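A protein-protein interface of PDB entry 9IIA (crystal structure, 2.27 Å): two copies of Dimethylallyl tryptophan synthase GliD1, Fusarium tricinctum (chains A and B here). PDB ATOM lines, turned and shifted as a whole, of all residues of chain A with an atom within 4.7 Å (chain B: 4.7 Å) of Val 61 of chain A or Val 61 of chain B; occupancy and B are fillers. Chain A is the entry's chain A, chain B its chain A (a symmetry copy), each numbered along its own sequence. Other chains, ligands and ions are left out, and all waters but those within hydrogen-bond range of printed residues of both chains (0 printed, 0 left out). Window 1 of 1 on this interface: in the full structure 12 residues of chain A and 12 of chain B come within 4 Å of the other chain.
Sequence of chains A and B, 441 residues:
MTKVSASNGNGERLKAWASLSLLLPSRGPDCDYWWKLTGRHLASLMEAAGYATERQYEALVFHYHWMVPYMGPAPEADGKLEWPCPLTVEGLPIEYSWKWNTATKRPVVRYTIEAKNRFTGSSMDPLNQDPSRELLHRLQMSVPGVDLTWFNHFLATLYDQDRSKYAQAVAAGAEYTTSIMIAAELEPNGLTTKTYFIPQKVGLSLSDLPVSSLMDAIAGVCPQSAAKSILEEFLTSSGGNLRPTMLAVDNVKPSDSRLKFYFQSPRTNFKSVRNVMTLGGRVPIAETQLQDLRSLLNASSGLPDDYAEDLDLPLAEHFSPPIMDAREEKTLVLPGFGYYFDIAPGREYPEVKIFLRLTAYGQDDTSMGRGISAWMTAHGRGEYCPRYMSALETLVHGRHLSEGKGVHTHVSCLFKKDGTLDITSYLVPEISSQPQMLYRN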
ATOM      1  N   LEU A  20       3.963   9.087  28.564  1.00  0.00           N
ATOM      2  CA  LEU A  20       5.180   8.751  27.833  1.00  0.00           C
ATOM      3  C   LEU A  20       5.262   9.485  26.503  1.00  0.00           C
ATOM      4  O   LEU A  20       6.345   9.927  26.102  1.00  0.00           O
ATOM      5  CB  LEU A  20       5.263   7.245  27.608  1.00  0.00           C
ATOM      6  CG  LEU A  20       6.201   6.506  28.546  1.00  0.00           C
ATOM      7  CD1 LEU A  20       6.167   5.031  28.207  1.00  0.00           C
ATOM      8  CD2 LEU A  20       7.610   7.074  28.409  1.00  0.00           C
ATOM      9  N   LEU A  23       6.743  12.927  26.998  1.00  0.00           N
ATOM     10  CA  LEU A  23       8.137  12.930  27.418  1.00  0.00           C
ATOM     11  C   LEU A  23       9.089  12.360  26.373  1.00  0.00           C
ATOM     12  O   LEU A  23      10.301  12.580  26.486  1.00  0.00           O
ATOM     13  CB  LEU A  23       8.320  12.124  28.708  1.00  0.00           C
ATOM     14  CG  LEU A  23       7.631  12.580  29.998  1.00  0.00           C
ATOM     15  CD1 LEU A  23       7.828  11.557  31.079  1.00  0.00           C
ATOM     16  CD2 LEU A  23       8.154  13.936  30.461  1.00  0.00           C
ATOM     17  N   LEU A  24       8.581  11.601  25.366  1.00  0.00           N
ATOM     18  CA  LEU A  24       9.505  10.981  24.412  1.00  0.00           C
ATOM     19  C   LEU A  24       9.585  11.829  23.159  1.00  0.00           C
ATOM     20  O   LEU A  24       8.546  12.158  22.573  1.00  0.00           O
ATOM     21  CB  LEU A  24       9.065   9.563  24.052  1.00  0.00           C
ATOM     22  CG  LEU A  24       9.116   8.563  25.211  1.00  0.00           C
ATOM     23  CD1 LEU A  24       8.553   7.217  24.795  1.00  0.00           C
ATOM     24  CD2 LEU A  24      10.522   8.402  25.779  1.00  0.00           C
ATOM     25  N   TYR A  57       4.672   1.172  31.054  1.00  0.00           N
ATOM     26  CA  TYR A  57       5.780   2.081  30.773  1.00  0.00           C
ATOM     27  C   TYR A  57       6.949   1.328  30.163  1.00  0.00           C
ATOM     28  O   TYR A  57       7.539   1.769  29.170  1.00  0.00           O
ATOM     29  CB  TYR A  57       6.242   2.784  32.054  1.00  0.00           C
ATOM     30  CG  TYR A  57       5.459   4.006  32.472  1.00  0.00           C
ATOM     31  CD1 TYR A  57       4.692   4.718  31.573  1.00  0.00           C
ATOM     32  CD2 TYR A  57       5.493   4.445  33.790  1.00  0.00           C
ATOM     33  CE1 TYR A  57       3.983   5.841  31.977  1.00  0.00           C
ATOM     34  CE2 TYR A  57       4.783   5.558  34.202  1.00  0.00           C
ATOM     35  CZ  TYR A  57       4.027   6.250  33.297  1.00  0.00           C
ATOM     36  OH  TYR A  57       3.325   7.360  33.715  1.00  0.00           O
ATOM     37  N   GLU A  58       7.297   0.185  30.754  1.00  0.00           N
ATOM     38  CA  GLU A  58       8.431  -0.594  30.266  1.00  0.00           C
ATOM     39  C   GLU A  58       8.206  -1.076  28.841  1.00  0.00           C
ATOM     40  O   GLU A  58       9.086  -0.928  27.981  1.00  0.00           O
ATOM     41  CB  GLU A  58       8.695  -1.770  31.200  1.00  0.00           C
ATOM     42  CG  GLU A  58       9.037  -1.322  32.597  1.00  0.00           C
ATOM     43  CD  GLU A  58       9.463  -2.461  33.494  1.00  0.00           C
ATOM     44  OE1 GLU A  58      10.369  -3.233  33.092  1.00  0.00           O
ATOM     45  OE2 GLU A  58       8.888  -2.579  34.601  1.00  0.00           O
ATOM     46  N   ALA A  59       7.030  -1.658  28.568  1.00  0.00           N
ATOM     47  CA  ALA A  59       6.740  -2.137  27.217  1.00  0.00           C
ATOM     48  C   ALA A  59       6.781  -0.997  26.209  1.00  0.00           C
ATOM     49  O   ALA A  59       7.363  -1.123  25.126  1.00  0.00           O
ATOM     50  CB  ALA A  59       5.376  -2.825  27.176  1.00  0.00           C
ATOM     51  N   LEU A  60       6.143   0.121  26.537  1.00  0.00           N
ATOM     52  CA  LEU A  60       6.092   1.231  25.595  1.00  0.00           C
ATOM     53  C   LEU A  60       7.475   1.837  25.388  1.00  0.00           C
ATOM     54  O   LEU A  60       7.843   2.196  24.267  1.00  0.00           O
ATOM     55  CB  LEU A  60       5.092   2.268  26.095  1.00  0.00           C
ATOM     56  CG  LEU A  60       3.625   1.870  25.955  1.00  0.00           C
ATOM     57  CD1 LEU A  60       2.747   2.847  26.742  1.00  0.00           C
ATOM     58  CD2 LEU A  60       3.214   1.828  24.492  1.00  0.00           C
ATOM     59  N   VAL A  61       8.266   1.925  26.457  1.00  0.00           N
ATOM     60  CA  VAL A  61       9.641   2.386  26.328  1.00  0.00           C
ATOM     61  C   VAL A  61      10.441   1.422  25.469  1.00  0.00           C
ATOM     62  O   VAL A  61      11.215   1.841  24.599  1.00  0.00           O
ATOM     63  CB  VAL A  61      10.264   2.571  27.727  1.00  0.00           C
ATOM     64  CG1 VAL A  61      11.749   2.343  27.711  1.00  0.00           C
ATOM     65  CG2 VAL A  61       9.961   3.973  28.239  1.00  0.00           C
ATOM     66  N   PHE A  62      10.273   0.113  25.701  1.00  0.00           N
ATOM     67  CA  PHE A  62      10.952  -0.870  24.866  1.00  0.00           C
ATOM     68  C   PHE A  62      10.502  -0.743  23.417  1.00  0.00           C
ATOM     69  O   PHE A  62      11.327  -0.774  22.497  1.00  0.00           O
ATOM     70  CB  PHE A  62      10.701  -2.284  25.392  1.00  0.00           C
ATOM     71  CG  PHE A  62      11.244  -3.360  24.497  1.00  0.00           C
ATOM     72  CD1 PHE A  62      12.579  -3.755  24.586  1.00  0.00           C
ATOM     73  CD2 PHE A  62      10.444  -3.936  23.535  1.00  0.00           C
ATOM     74  CE1 PHE A  62      13.091  -4.719  23.735  1.00  0.00           C
ATOM     75  CE2 PHE A  62      10.947  -4.919  22.691  1.00  0.00           C
ATOM     76  CZ  PHE A  62      12.270  -5.304  22.788  1.00  0.00           C
ATOM     77  N   HIS A  63       9.195  -0.589  23.198  1.00  0.00           N
ATOM     78  CA  HIS A  63       8.683  -0.417  21.844  1.00  0.00           C
ATOM     79  C   HIS A  63       9.334   0.784  21.164  1.00  0.00           C
ATOM     80  O   HIS A  63       9.799   0.689  20.021  1.00  0.00           O
ATOM     81  CB  HIS A  63       7.158  -0.260  21.893  1.00  0.00           C
ATOM     82  CG  HIS A  63       6.498  -0.224  20.548  1.00  0.00           C
ATOM     83  ND1 HIS A  63       6.706  -1.193  19.588  1.00  0.00           N
ATOM     84  CD2 HIS A  63       5.614   0.651  20.010  1.00  0.00           C
ATOM     85  CE1 HIS A  63       5.987  -0.911  18.514  1.00  0.00           C
ATOM     86  NE2 HIS A  63       5.312   0.202  18.744  1.00  0.00           N
ATOM     87  N   TYR A  64       9.375   1.927  21.862  1.00  0.00           N
ATOM     88  CA  TYR A  64       9.883   3.164  21.265  1.00  0.00           C
ATOM     89  C   TYR A  64      11.327   3.009  20.817  1.00  0.00           C
ATOM     90  O   TYR A  64      11.680   3.392  19.695  1.00  0.00           O
ATOM     91  CB  TYR A  64       9.749   4.316  22.265  1.00  0.00           C
ATOM     92  CG  TYR A  64      10.366   5.664  21.868  1.00  0.00           C
ATOM     93  CD1 TYR A  64      11.705   5.957  22.138  1.00  0.00           C
ATOM     94  CD2 TYR A  64       9.584   6.661  21.273  1.00  0.00           C
ATOM     95  CE1 TYR A  64      12.267   7.204  21.806  1.00  0.00           C
ATOM     96  CE2 TYR A  64      10.128   7.908  20.935  1.00  0.00           C
ATOM     97  CZ  TYR A  64      11.472   8.170  21.200  1.00  0.00           C
ATOM     98  OH  TYR A  64      12.005   9.396  20.866  1.00  0.00           O
ATOM     99  N   HIS A  65      12.167   2.413  21.656  1.00  0.00           N
ATOM    100  CA  HIS A  65      13.597   2.398  21.365  1.00  0.00           C
ATOM    101  C   HIS A  65      14.041   1.228  20.508  1.00  0.00           C
ATOM    102  O   HIS A  65      14.928   1.390  19.673  1.00  0.00           O
ATOM    103  CB  HIS A  65      14.398   2.372  22.655  1.00  0.00           C
ATOM    104  CG  HIS A  65      14.406   3.682  23.360  1.00  0.00           C
ATOM    105  ND1 HIS A  65      13.437   4.037  24.277  1.00  0.00           N
ATOM    106  CD2 HIS A  65      15.232   4.747  23.243  1.00  0.00           C
ATOM    107  CE1 HIS A  65      13.689   5.253  24.722  1.00  0.00           C
ATOM    108  NE2 HIS A  65      14.774   5.703  24.112  1.00  0.00           N
ATOM    109  N   LEU B  20      14.910   0.454  33.849  1.00  0.00           N
ATOM    110  CA  LEU B  20      15.056   1.393  32.741  1.00  0.00           C
ATOM    111  C   LEU B  20      16.433   1.305  32.102  1.00  0.00           C
ATOM    112  O   LEU B  20      16.558   1.398  30.875  1.00  0.00           O
ATOM    113  CB  LEU B  20      14.786   2.817  33.217  1.00  0.00           C
ATOM    114  CG  LEU B  20      13.414   3.364  32.864  1.00  0.00           C
ATOM    115  CD1 LEU B  20      13.296   4.771  33.407  1.00  0.00           C
ATOM    116  CD2 LEU B  20      13.230   3.337  31.351  1.00  0.00           C
ATOM    117  N   LEU B  23      16.502  -1.451  29.517  1.00  0.00           N
ATOM    118  CA  LEU B  23      15.658  -1.210  28.356  1.00  0.00           C
ATOM    119  C   LEU B  23      16.106  -0.021  27.513  1.00  0.00           C
ATOM    120  O   LEU B  23      15.661   0.098  26.366  1.00  0.00           O
ATOM    121  CB  LEU B  23      14.205  -0.966  28.777  1.00  0.00           C
ATOM    122  CG  LEU B  23      13.418  -2.076  29.480  1.00  0.00           C
ATOM    123  CD1 LEU B  23      12.083  -1.556  29.932  1.00  0.00           C
ATOM    124  CD2 LEU B  23      13.225  -3.286  28.570  1.00  0.00           C
ATOM    125  N   LEU B  24      16.955   0.889  28.060  1.00  0.00           N
ATOM    126  CA  LEU B  24      17.316   2.077  27.282  1.00  0.00           C
ATOM    127  C   LEU B  24      18.658   1.858  26.616  1.00  0.00           C
ATOM    128  O   LEU B  24      19.629   1.499  27.293  1.00  0.00           O
ATOM    129  CB  LEU B  24      17.369   3.324  28.162  1.00  0.00           C
ATOM    130  CG  LEU B  24      16.022   3.750  28.752  1.00  0.00           C
ATOM    131  CD1 LEU B  24      16.188   4.921  29.703  1.00  0.00           C
ATOM    132  CD2 LEU B  24      14.993   4.078  27.676  1.00  0.00           C
ATOM    133  N   TYR B  57      10.119   6.563  36.862  1.00  0.00           N
ATOM    134  CA  TYR B  57      10.264   6.209  35.453  1.00  0.00           C
ATOM    135  C   TYR B  57      10.196   7.449  34.579  1.00  0.00           C
ATOM    136  O   TYR B  57      11.016   7.632  33.672  1.00  0.00           O
ATOM    137  CB  TYR B  57       9.170   5.226  35.026  1.00  0.00           C
ATOM    138  CG  TYR B  57       9.418   3.767  35.329  1.00  0.00           C
ATOM    139  CD1 TYR B  57      10.689   3.278  35.548  1.00  0.00           C
ATOM    140  CD2 TYR B  57       8.356   2.874  35.398  1.00  0.00           C
ATOM    141  CE1 TYR B  57      10.896   1.932  35.821  1.00  0.00           C
ATOM    142  CE2 TYR B  57       8.553   1.534  35.677  1.00  0.00           C
ATOM    143  CZ  TYR B  57       9.820   1.068  35.892  1.00  0.00           C
ATOM    144  OH  TYR B  57      10.008  -0.269  36.167  1.00  0.00           O
ATOM    145  N   GLU B  58       9.214   8.311  34.843  1.00  0.00           N
ATOM    146  CA  GLU B  58       9.040   9.515  34.035  1.00  0.00           C
ATOM    147  C   GLU B  58      10.250  10.433  34.133  1.00  0.00           C
ATOM    148  O   GLU B  58      10.766  10.903  33.109  1.00  0.00           O
ATOM    149  CB  GLU B  58       7.771  10.246  34.457  1.00  0.00           C
ATOM    150  CG  GLU B  58       6.537   9.404  34.263  1.00  0.00           C
ATOM    151  CD  GLU B  58       5.256  10.165  34.518  1.00  0.00           C
ATOM    152  OE1 GLU B  58       5.085  11.262  33.930  1.00  0.00           O
ATOM    153  OE2 GLU B  58       4.426   9.660  35.308  1.00  0.00           O
ATOM    154  N   ALA B  59      10.719  10.702  35.359  1.00  0.00           N
ATOM    155  CA  ALA B  59      11.885  11.569  35.529  1.00  0.00           C
ATOM    156  C   ALA B  59      13.108  10.988  34.832  1.00  0.00           C
ATOM    157  O   ALA B  59      13.844  11.698  34.138  1.00  0.00           O
ATOM    158  CB  ALA B  59      12.179  11.783  37.013  1.00  0.00           C
ATOM    159  N   LEU B  60      13.357   9.698  35.028  1.00  0.00           N
ATOM    160  CA  LEU B  60      14.543   9.090  34.441  1.00  0.00           C
ATOM    161  C   LEU B  60      14.440   9.051  32.920  1.00  0.00           C
ATOM    162  O   LEU B  60      15.425   9.290  32.217  1.00  0.00           O
ATOM    163  CB  LEU B  60      14.736   7.697  35.028  1.00  0.00           C
ATOM    164  CG  LEU B  60      15.239   7.668  36.469  1.00  0.00           C
ATOM    165  CD1 LEU B  60      15.117   6.248  37.030  1.00  0.00           C
ATOM    166  CD2 LEU B  60      16.674   8.162  36.551  1.00  0.00           C
ATOM    167  N   VAL B  61      13.244   8.784  32.399  1.00  0.00           N
ATOM    168  CA  VAL B  61      13.032   8.837  30.958  1.00  0.00           C
ATOM    169  C   VAL B  61      13.248  10.250  30.447  1.00  0.00           C
ATOM    170  O   VAL B  61      13.889  10.458  29.409  1.00  0.00           O
ATOM    171  CB  VAL B  61      11.625   8.304  30.617  1.00  0.00           C
ATOM    172  CG1 VAL B  61      11.072   8.946  29.375  1.00  0.00           C
ATOM    173  CG2 VAL B  61      11.680   6.793  30.439  1.00  0.00           C
ATOM    174  N   PHE B  62      12.712  11.248  31.164  1.00  0.00           N
ATOM    175  CA  PHE B  62      12.943  12.634  30.773  1.00  0.00           C
ATOM    176  C   PHE B  62      14.428  12.964  30.825  1.00  0.00           C
ATOM    177  O   PHE B  62      14.964  13.598  29.910  1.00  0.00           O
ATOM    178  CB  PHE B  62      12.142  13.582  31.666  1.00  0.00           C
ATOM    179  CG  PHE B  62      12.444  15.032  31.421  1.00  0.00           C
ATOM    180  CD1 PHE B  62      11.799  15.732  30.401  1.00  0.00           C
ATOM    181  CD2 PHE B  62      13.405  15.680  32.166  1.00  0.00           C
ATOM    182  CE1 PHE B  62      12.105  17.059  30.149  1.00  0.00           C
ATOM    183  CE2 PHE B  62      13.702  17.016  31.931  1.00  0.00           C
ATOM    184  CZ  PHE B  62      13.057  17.702  30.920  1.00  0.00           C
ATOM    185  N   HIS B  63      15.109  12.534  31.888  1.00  0.00           N
ATOM    186  CA  HIS B  63      16.544  12.769  31.999  1.00  0.00           C
ATOM    187  C   HIS B  63      17.286  12.186  30.800  1.00  0.00           C
ATOM    188  O   HIS B  63      18.123  12.857  30.186  1.00  0.00           O
ATOM    189  CB  HIS B  63      17.059  12.166  33.311  1.00  0.00           C
ATOM    190  CG  HIS B  63      18.494  12.473  33.610  1.00  0.00           C
ATOM    191  ND1 HIS B  63      18.999  13.757  33.610  1.00  0.00           N
ATOM    192  CD2 HIS B  63      19.530  11.666  33.943  1.00  0.00           C
ATOM    193  CE1 HIS B  63      20.285  13.726  33.918  1.00  0.00           C
ATOM    194  NE2 HIS B  63      20.634  12.469  34.130  1.00  0.00           N
ATOM    195  N   TYR B  64      16.983  10.926  30.456  1.00  0.00           N
ATOM    196  CA  TYR B  64      17.709  10.236  29.387  1.00  0.00           C
ATOM    197  C   TYR B  64      17.578  10.972  28.065  1.00  0.00           C
ATOM    198  O   TYR B  64      18.575  11.187  27.366  1.00  0.00           O
ATOM    199  CB  TYR B  64      17.198   8.798  29.258  1.00  0.00           C
ATOM    200  CG  TYR B  64      17.741   7.963  28.090  1.00  0.00           C
ATOM    201  CD1 TYR B  64      17.135   7.995  26.832  1.00  0.00           C
ATOM    202  CD2 TYR B  64      18.829   7.102  28.273  1.00  0.00           C
ATOM    203  CE1 TYR B  64      17.608   7.205  25.767  1.00  0.00           C
ATOM    204  CE2 TYR B  64      19.314   6.311  27.222  1.00  0.00           C
ATOM    205  CZ  TYR B  64      18.702   6.371  25.971  1.00  0.00           C
ATOM    206  OH  TYR B  64      19.181   5.594  24.940  1.00  0.00           O
ATOM    207  N   HIS B  65      16.370  11.405  27.722  1.00  0.00           N
ATOM    208  CA  HIS B  65      16.145  11.953  26.389  1.00  0.00           C
ATOM    209  C   HIS B  65      16.418  13.440  26.278  1.00  0.00           C
ATOM    210  O   HIS B  65      16.915  13.891  25.248  1.00  0.00           O
ATOM    211  CB  HIS B  65      14.713  11.700  25.949  1.00  0.00           C
ATOM    212  CG  HIS B  65      14.464  10.283  25.568  1.00  0.00           C
ATOM    213  ND1 HIS B  65      14.074   9.327  26.485  1.00  0.00           N
ATOM    214  CD2 HIS B  65      14.603   9.645  24.384  1.00  0.00           C
ATOM    215  CE1 HIS B  65      13.948   8.166  25.870  1.00  0.00           C
ATOM    216  NE2 HIS B  65      14.261   8.335  24.595  1.00  0.00           N
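Val 61 of chain A touches just these residues of chain B: Leu 24 (3.7 Å) and Val 61 (3.97 Å). Val 61 of chain B touches two residues of chain A. Printed residues of chain B within 4 Å of His 65 of chain A: Leu 24, Tyr 64 and His 65. Printed residues of chain A within 4 Å of Tyr 57 of chain B: Tyr 57 (3.6 Å) and Glu 58 (3.0 Å). Of the printed residues of chain B, Leu 23 of chain A touches Glu 58 (3.6 Å). Leu 20 of chain B touches none of the printed residues of chain A. The nearest residue of chain B that does not touch Val 61 of chain A is Leu 20 of chain B (4.1 Å).
The side-chain carboxylate (OE2) of Glu 58 of chain B sits at hydrogen-bond distance from the side-chain hydroxyl (OH) of Tyr 57 of chain A, 3.0 Å away. The side-chain hydroxyl (OH) of Tyr 57 of chain B is in hydrogen-bond range of the side-chain carboxylate (OE2) of Glu 58 of chain A (3.0 Å). NE2 of His 65 of chain A is in hydrogen-bond range of NE2 of His 65 of chain B (2.7 Å).
Leu 24 of chain A touches Val 61 of chain B, and with the chains exchanged Val 61 of chain A touches Leu 24 of chain B. Tyr 57 of chain B touches its own counterpart, Tyr 57 of chain A. Tyr 57 of chain A touches Glu 58 of chain B, and with the chains exchanged Glu 58 of chain A touches Tyr 57 of chain B. Val 61 of chain A touches its own counterpart, Val 61 of chain B. Positions printed for both chains: 20, 23, 24, 57, 58, 59, 60, 61, 62, 63, 64 and 65.
The backbone carbonyl oxygen of Val 61 of chain B is in hydrogen-bond range of a ring nitrogen (ND1) of His 65 of chain B (3.1 Å). ND1 of His 65 of chain A sits at hydrogen-bond distance from O of Val 61 of chain A, at 3.1 Å.
Of the 12 printed residues of chain A, 7 touch a printed residue of chain B. Hydrophobic or aromatic side chains of chain A that line the printed part of chain B: Leu 23, Leu 24, Tyr 57, Val 61, Tyr 64 and His 65. Printed residues of chain B that touch a printed residue of chain A: Leu 23, Leu 24, Tyr 57, Glu 58, Val 61, Tyr 64 and His 65. Hydrophobic or aromatic side chains of chain B that line the printed part of chain A: Leu 23, Leu 24, Tyr 57, Val 61, Tyr 64 and His 65.
Among the printed residues, pairs that only touch across the chains: Leu 24 of chain A with His 65 of chain B (3.4 Å), His 65 of chain A with Leu 24 of chain B (3.4 Å), His 65 of chain A with Tyr 64 of chain B (3.6 Å), Tyr 64 of chain A with His 65 of chain B (3.6 Å), Glu 58 of chain A with Leu 23 of chain B (3.6 Å), Leu 23 of chain A with Glu 58 of chain B (3.6 Å), Tyr 57 of chain A with Tyr 57 of chain B (3.6 Å), Leu 24 of chain A with Val 61 of chain B (3.7 Å), Val 61 of chain A with Leu 24 of chain B (3.7 Å) and Val 61 of chain A with Val 61 of chain B (3.97 Å).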
